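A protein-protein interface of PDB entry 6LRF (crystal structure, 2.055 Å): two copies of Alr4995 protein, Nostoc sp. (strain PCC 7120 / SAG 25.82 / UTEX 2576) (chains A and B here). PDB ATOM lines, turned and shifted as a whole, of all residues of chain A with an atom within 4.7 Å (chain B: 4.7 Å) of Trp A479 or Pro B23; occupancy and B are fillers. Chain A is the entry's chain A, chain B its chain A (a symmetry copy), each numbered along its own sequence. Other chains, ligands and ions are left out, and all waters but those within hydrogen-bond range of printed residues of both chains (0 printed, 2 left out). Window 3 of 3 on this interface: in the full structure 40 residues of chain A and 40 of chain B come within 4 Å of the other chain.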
ATOM      1  N   GLU A 475     -23.053  -6.679 -13.420  1.00  0.00           N
ATOM      2  CA  GLU A 475     -22.515  -5.326 -13.441  1.00  0.00           C
ATOM      3  C   GLU A 475     -22.070  -4.905 -14.848  1.00  0.00           C
ATOM      4  O   GLU A 475     -22.437  -3.842 -15.337  1.00  0.00           O
ATOM      5  CB  GLU A 475     -21.342  -5.232 -12.464  1.00  0.00           C
ATOM      6  CG  GLU A 475     -20.694  -3.857 -12.355  1.00  0.00           C
ATOM      7  CD  GLU A 475     -19.503  -3.849 -11.384  1.00  0.00           C
ATOM      8  OE1 GLU A 475     -18.506  -4.561 -11.652  1.00  0.00           O
ATOM      9  OE2 GLU A 475     -19.571  -3.148 -10.346  1.00  0.00           O
ATOM     10  N   GLN A 476     -21.294  -5.757 -15.496  1.00  0.00           N
ATOM     11  CA  GLN A 476     -20.789  -5.471 -16.833  1.00  0.00           C
ATOM     12  C   GLN A 476     -21.903  -5.425 -17.885  1.00  0.00           C
ATOM     13  O   GLN A 476     -21.943  -4.523 -18.730  1.00  0.00           O
ATOM     14  CB  GLN A 476     -19.744  -6.520 -17.230  1.00  0.00           C
ATOM     15  CG  GLN A 476     -19.458  -6.558 -18.737  1.00  0.00           C
ATOM     16  CD  GLN A 476     -18.626  -7.759 -19.160  1.00  0.00           C
ATOM     17  OE1 GLN A 476     -18.194  -8.561 -18.322  1.00  0.00           O
ATOM     18  NE2 GLN A 476     -18.401  -7.894 -20.467  1.00  0.00           N
ATOM     19  N   VAL A 477     -22.801  -6.406 -17.842  1.00  0.00           N
ATOM     20  CA  VAL A 477     -23.869  -6.507 -18.833  1.00  0.00           C
ATOM     21  C   VAL A 477     -24.868  -5.360 -18.675  1.00  0.00           C
ATOM     22  O   VAL A 477     -25.325  -4.788 -19.666  1.00  0.00           O
ATOM     23  CB  VAL A 477     -24.596  -7.885 -18.737  1.00  0.00           C
ATOM     24  CG1 VAL A 477     -25.809  -7.926 -19.650  1.00  0.00           C
ATOM     25  CG2 VAL A 477     -23.638  -9.002 -19.107  1.00  0.00           C
ATOM     26  N   ALA A 478     -25.186  -4.991 -17.435  1.00  0.00           N
ATOM     27  CA  ALA A 478     -26.098  -3.866 -17.226  1.00  0.00           C
ATOM     28  C   ALA A 478     -25.527  -2.572 -17.785  1.00  0.00           C
ATOM     29  O   ALA A 478     -26.233  -1.799 -18.425  1.00  0.00           O
ATOM     30  CB  ALA A 478     -26.407  -3.687 -15.760  1.00  0.00           C
ATOM     31  N   TRP A 479     -24.247  -2.340 -17.511  1.00  0.00           N
ATOM     32  CA  TRP A 479     -23.557  -1.144 -17.986  1.00  0.00           C
ATOM     33  C   TRP A 479     -23.615  -1.103 -19.512  1.00  0.00           C
ATOM     34  O   TRP A 479     -23.969  -0.082 -20.101  1.00  0.00           O
ATOM     35  CB  TRP A 479     -22.102  -1.129 -17.478  1.00  0.00           C
ATOM     36  CG  TRP A 479     -21.282  -0.016 -18.037  1.00  0.00           C
ATOM     37  CD1 TRP A 479     -21.297   1.290 -17.645  1.00  0.00           C
ATOM     38  CD2 TRP A 479     -20.316  -0.110 -19.096  1.00  0.00           C
ATOM     39  NE1 TRP A 479     -20.407   2.021 -18.408  1.00  0.00           N
ATOM     40  CE2 TRP A 479     -19.795   1.178 -19.302  1.00  0.00           C
ATOM     41  CE3 TRP A 479     -19.857  -1.157 -19.896  1.00  0.00           C
ATOM     42  CZ2 TRP A 479     -18.823   1.443 -20.268  1.00  0.00           C
ATOM     43  CZ3 TRP A 479     -18.890  -0.893 -20.859  1.00  0.00           C
ATOM     44  CH2 TRP A 479     -18.392   0.395 -21.040  1.00  0.00           C
ATOM     45  N   GLU A 480     -23.288  -2.228 -20.148  1.00  0.00           N
ATOM     46  CA  GLU A 480     -23.313  -2.319 -21.613  1.00  0.00           C
ATOM     47  C   GLU A 480     -24.712  -2.135 -22.195  1.00  0.00           C
ATOM     48  O   GLU A 480     -24.885  -1.451 -23.199  1.00  0.00           O
ATOM     49  CB  GLU A 480     -22.729  -3.652 -22.072  1.00  0.00           C
ATOM     50  CG  GLU A 480     -21.324  -3.529 -22.651  1.00  0.00           C
ATOM     51  CD  GLU A 480     -20.577  -4.858 -22.722  1.00  0.00           C
ATOM     52  OE1 GLU A 480     -21.038  -5.852 -22.101  1.00  0.00           O
ATOM     53  OE2 GLU A 480     -19.515  -4.900 -23.385  1.00  0.00           O
ATOM     54  N   LEU A 481     -25.717  -2.718 -21.556  1.00  0.00           N
ATOM     55  CA  LEU A 481     -27.092  -2.558 -22.037  1.00  0.00           C
ATOM     56  C   LEU A 481     -27.538  -1.103 -22.013  1.00  0.00           C
ATOM     57  O   LEU A 481     -28.141  -0.621 -22.964  1.00  0.00           O
ATOM     58  CB  LEU A 481     -28.056  -3.391 -21.196  1.00  0.00           C
ATOM     59  CG  LEU A 481     -28.171  -4.848 -21.584  1.00  0.00           C
ATOM     60  CD1 LEU A 481     -29.057  -5.560 -20.566  1.00  0.00           C
ATOM     61  CD2 LEU A 481     -28.764  -4.933 -22.983  1.00  0.00           C
ATOM     62  N   ARG A 482     -27.251  -0.411 -20.915  1.00  0.00           N
ATOM     63  CA  ARG A 482     -27.652   0.990 -20.761  1.00  0.00           C
ATOM     64  C   ARG A 482     -26.885   1.824 -21.762  1.00  0.00           C
ATOM     65  O   ARG A 482     -27.437   2.721 -22.398  1.00  0.00           O
ATOM     66  CB  ARG A 482     -27.410   1.486 -19.330  1.00  0.00           C
ATOM     67  CG  ARG A 482     -27.520   3.020 -19.122  1.00  0.00           C
ATOM     68  CD  ARG A 482     -27.481   3.374 -17.627  1.00  0.00           C
ATOM     69  NE  ARG A 482     -26.912   4.695 -17.306  1.00  0.00           N
ATOM     70  CZ  ARG A 482     -25.604   4.947 -17.179  1.00  0.00           C
ATOM     71  NH1 ARG A 482     -24.703   3.980 -17.371  1.00  0.00           N
ATOM     72  NH2 ARG A 482     -25.186   6.174 -16.868  1.00  0.00           N
ATOM     73  N   LYS A 483     -25.611   1.488 -21.923  1.00  0.00           N
ATOM     74  CA  LYS A 483     -24.765   2.181 -22.877  1.00  0.00           C
ATOM     75  C   LYS A 483     -25.293   2.025 -24.306  1.00  0.00           C
ATOM     76  O   LYS A 483     -25.429   3.004 -25.038  1.00  0.00           O
ATOM     77  CB  LYS A 483     -23.343   1.652 -22.754  1.00  0.00           C
ATOM     78  CG  LYS A 483     -22.340   2.292 -23.648  1.00  0.00           C
ATOM     79  CD  LYS A 483     -20.966   1.737 -23.289  1.00  0.00           C
ATOM     80  CE  LYS A 483     -19.898   2.512 -23.976  1.00  0.00           C
ATOM     81  NZ  LYS A 483     -20.087   2.366 -25.426  1.00  0.00           N
ATOM     82  N   LEU A 694     -28.051   2.359 -11.831  1.00  0.00           N
ATOM     83  CA  LEU A 694     -27.449   3.303 -12.774  1.00  0.00           C
ATOM     84  C   LEU A 694     -28.424   4.420 -13.094  1.00  0.00           C
ATOM     85  O   LEU A 694     -28.043   5.439 -13.668  1.00  0.00           O
ATOM     86  CB  LEU A 694     -27.028   2.589 -14.060  1.00  0.00           C
ATOM     87  CG  LEU A 694     -26.106   1.384 -13.875  1.00  0.00           C
ATOM     88  CD1 LEU A 694     -26.120   0.530 -15.123  1.00  0.00           C
ATOM     89  CD2 LEU A 694     -24.678   1.808 -13.535  1.00  0.00           C
ATOM     90  N   ASN B  22     -10.843   1.970 -26.308  1.00  0.00           N
ATOM     91  CA  ASN B  22     -11.273   1.690 -24.923  1.00  0.00           C
ATOM     92  C   ASN B  22     -12.758   1.288 -24.949  1.00  0.00           C
ATOM     93  O   ASN B  22     -13.412   1.427 -25.984  1.00  0.00           O
ATOM     94  CB  ASN B  22     -10.973   2.898 -23.986  1.00  0.00           C
ATOM     95  CG  ASN B  22     -11.830   4.123 -24.271  1.00  0.00           C
ATOM     96  OD1 ASN B  22     -13.044   4.050 -24.216  1.00  0.00           O
ATOM     97  ND2 ASN B  22     -11.186   5.278 -24.515  1.00  0.00           N
ATOM     98  N   PRO B  23     -13.290   0.732 -23.844  1.00  0.00           N
ATOM     99  CA  PRO B  23     -14.648   0.160 -23.918  1.00  0.00           C
ATOM    100  C   PRO B  23     -15.758   1.201 -24.062  1.00  0.00           C
ATOM    101  O   PRO B  23     -16.888   0.867 -24.408  1.00  0.00           O
ATOM    102  CB  PRO B  23     -14.798  -0.578 -22.569  1.00  0.00           C
ATOM    103  CG  PRO B  23     -13.441  -0.766 -22.071  1.00  0.00           C
ATOM    104  CD  PRO B  23     -12.621   0.379 -22.579  1.00  0.00           C
ATOM    105  N   TRP B  24     -15.443   2.460 -23.787  1.00  0.00           N
ATOM    106  CA  TRP B  24     -16.446   3.497 -23.906  1.00  0.00           C
ATOM    107  C   TRP B  24     -16.695   3.822 -25.377  1.00  0.00           C
ATOM    108  O   TRP B  24     -17.817   4.101 -25.764  1.00  0.00           O
ATOM    109  CB  TRP B  24     -16.012   4.755 -23.140  1.00  0.00           C
ATOM    110  CG  TRP B  24     -15.823   4.502 -21.671  1.00  0.00           C
ATOM    111  CD1 TRP B  24     -14.693   4.041 -21.059  1.00  0.00           C
ATOM    112  CD2 TRP B  24     -16.807   4.658 -20.638  1.00  0.00           C
ATOM    113  NE1 TRP B  24     -14.905   3.917 -19.698  1.00  0.00           N
ATOM    114  CE2 TRP B  24     -16.194   4.290 -19.415  1.00  0.00           C
ATOM    115  CE3 TRP B  24     -18.141   5.094 -20.624  1.00  0.00           C
ATOM    116  CZ2 TRP B  24     -16.869   4.338 -18.190  1.00  0.00           C
ATOM    117  CZ3 TRP B  24     -18.820   5.129 -19.406  1.00  0.00           C
ATOM    118  CH2 TRP B  24     -18.180   4.760 -18.207  1.00  0.00           C
ATOM    119  N   MET B  25     -15.637   3.795 -26.180  1.00  0.00           N
ATOM    120  CA  MET B  25     -15.717   4.086 -27.619  1.00  0.00           C
ATOM    121  C   MET B  25     -16.498   3.017 -28.388  1.00  0.00           C
ATOM    122  O   MET B  25     -16.998   3.266 -29.493  1.00  0.00           O
ATOM    123  CB  MET B  25     -14.310   4.204 -28.222  1.00  0.00           C
ATOM    124  CG  MET B  25     -13.493   5.403 -27.749  1.00  0.00           C
ATOM    125  SD  MET B  25     -11.849   5.560 -28.765  1.00  0.00           S
ATOM    126  CE  MET B  25     -10.854   6.768 -27.569  1.00  0.00           C
ATOM    127  N   GLU B  26     -16.595   1.821 -27.814  1.00  0.00           N
ATOM    128  CA  GLU B  26     -17.248   0.704 -28.498  1.00  0.00           C
ATOM    129  C   GLU B  26     -18.723   1.036 -28.750  1.00  0.00           C
ATOM    130  O   GLU B  26     -19.454   1.389 -27.827  1.00  0.00           O
ATOM    131  CB  GLU B  26     -17.093  -0.581 -27.677  1.00  0.00           C
ATOM    132  CG  GLU B  26     -17.625  -1.851 -28.351  1.00  0.00           C
ATOM    133  CD  GLU B  26     -16.914  -2.178 -29.663  1.00  0.00           C
ATOM    134  OE1 GLU B  26     -15.817  -2.784 -29.616  1.00  0.00           O
ATOM    135  OE2 GLU B  26     -17.453  -1.820 -30.743  1.00  0.00           O
ATOM    136  N   GLU B 164     -11.418  -2.663 -17.028  1.00  0.00           N
ATOM    137  CA  GLU B 164     -11.097  -2.111 -18.340  1.00  0.00           C
ATOM    138  C   GLU B 164     -11.832  -0.802 -18.670  1.00  0.00           C
ATOM    139  O   GLU B 164     -11.365   0.001 -19.500  1.00  0.00           O
ATOM    140  CB  GLU B 164     -11.395  -3.160 -19.429  1.00  0.00           C
ATOM    141  CG  GLU B 164     -10.328  -3.202 -20.529  1.00  0.00           C
ATOM    142  CD  GLU B 164     -10.881  -3.629 -21.884  1.00  0.00           C
ATOM    143  OE1 GLU B 164     -11.897  -4.366 -21.915  1.00  0.00           O
ATOM    144  OE2 GLU B 164     -10.300  -3.204 -22.914  1.00  0.00           O
ATOM    145  N   ARG B 165     -12.974  -0.583 -18.037  1.00  0.00           N
ATOM    146  CA  ARG B 165     -13.688   0.698 -18.194  1.00  0.00           C
ATOM    147  C   ARG B 165     -12.946   1.853 -17.538  1.00  0.00           C
ATOM    148  O   ARG B 165     -13.103   3.024 -17.929  1.00  0.00           O
ATOM    149  CB  ARG B 165     -15.084   0.611 -17.597  1.00  0.00           C
ATOM    150  CG  ARG B 165     -15.877  -0.598 -18.119  1.00  0.00           C
ATOM    151  CD  ARG B 165     -17.165  -0.714 -17.367  1.00  0.00           C
ATOM    152  NE  ARG B 165     -16.923  -1.022 -15.961  1.00  0.00           N
ATOM    153  CZ  ARG B 165     -17.851  -0.951 -15.017  1.00  0.00           C
ATOM    154  NH1 ARG B 165     -19.078  -0.573 -15.339  1.00  0.00           N
ATOM    155  NH2 ARG B 165     -17.550  -1.256 -13.759  1.00  0.00           N
ATOM    156  N   TYR B 167      -9.607   2.656 -17.316  1.00  0.00           N
ATOM    157  CA  TYR B 167      -8.361   2.240 -17.945  1.00  0.00           C
ATOM    158  C   TYR B 167      -7.201   3.247 -17.734  1.00  0.00           C
ATOM    159  O   TYR B 167      -6.032   2.922 -17.991  1.00  0.00           O
ATOM    160  CB  TYR B 167      -8.618   2.008 -19.448  1.00  0.00           C
ATOM    161  CG  TYR B 167      -9.054   3.265 -20.160  1.00  0.00           C
ATOM    162  CD1 TYR B 167     -10.391   3.682 -20.146  1.00  0.00           C
ATOM    163  CD2 TYR B 167      -8.116   4.085 -20.789  1.00  0.00           C
ATOM    164  CE1 TYR B 167     -10.779   4.893 -20.768  1.00  0.00           C
ATOM    165  CE2 TYR B 167      -8.492   5.280 -21.418  1.00  0.00           C
ATOM    166  CZ  TYR B 167      -9.828   5.676 -21.408  1.00  0.00           C
ATOM    167  OH  TYR B 167     -10.187   6.875 -22.028  1.00  0.00           O
ATOM    168  N   VAL B 214     -19.402   5.315 -13.040  1.00  0.00           N
ATOM    169  CA  VAL B 214     -19.647   5.237 -14.487  1.00  0.00           C
ATOM    170  C   VAL B 214     -20.130   6.577 -15.078  1.00  0.00           C
ATOM    171  O   VAL B 214     -20.292   6.700 -16.290  1.00  0.00           O
ATOM    172  CB  VAL B 214     -20.656   4.108 -14.846  1.00  0.00           C
ATOM    173  CG1 VAL B 214     -20.183   2.785 -14.277  1.00  0.00           C
ATOM    174  CG2 VAL B 214     -22.062   4.434 -14.348  1.00  0.00           C
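No position is printed for both chains.
Of the 8 pairs that touch across the chains among the printed residues, none has its exchanged pair printed and touching as well.
Trp A479 touches Pro B23 (CH2 to O, 3.7 Å).
Trp A479 touches Trp B24.
NH1 of Arg B165 touches CG of Trp A479, at 3.5 Å.
Trp A479 touches Val B214.
Pro B23 touches Lys A483.
Leu A694 touches Val B214.
Of the 10 printed residues of chain A, 3 touch a printed residue of chain B.
Of the 9 printed residues of chain B, 5 touch a printed residue of chain A.
Printed residues of chain B that touch a printed residue of chain A: Pro B23, Trp B24, Glu B26, Arg B165 and Val B214.
Hydrophobic or aromatic side chains of chain B that line the printed part of chain A: Trp B24 and Val B214.
Among the printed residues, no Asp or Glu carboxylate lies within 4 Å of a Lys or Arg side-chain nitrogen of the other chain.
The side-chain amino group (NZ) of Lys A483 lies within hydrogen-bond range of the backbone carbonyl oxygen (O) of Trp B24 (2.9 Å).
The backbone carbonyl oxygen (O) of Glu B26 is in hydrogen-bond range of the side-chain amino group (NZ) of Lys A483 (2.7 Å).
Of chain B, only Pro B23 (3.7 Å), Trp B24 (3.5 Å), Arg B165 (3.5 Å) and Val B214 (3.8 Å) come within 4 Å of Trp A479.
Arg A482 touches none of the printed residues of chain B.
Of the printed residues of chain B, Lys A483 touches Pro B23 (3.5 Å), Trp B24 (2.9 Å) and Glu B26 (2.7 Å).
Of the printed residues of chain B, Leu A694 touches Val B214 (3.8 Å).
Of the printed residues of chain A, Trp B24 touches Trp A479 and Lys A483.
Of the printed residues of chain A, Glu B26 touches Lys A483 (2.7 Å).
Tyr B167 touches none of the printed residues of chain A.
Printed residues of chain A within 4 Å of Val B214: Trp A479 (3.8 Å) and Leu A694 (3.8 Å).
The nearest printed residue of chain B that does not touch Leu A694 is Arg B165 (6.3 Å).
O of Arg B165 is in hydrogen-bond range of NE1 of Trp B24 (2.7 Å).
OD1 of Asn B22 lies within hydrogen-bond range of N of Trp B24, at 2.9 Å.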
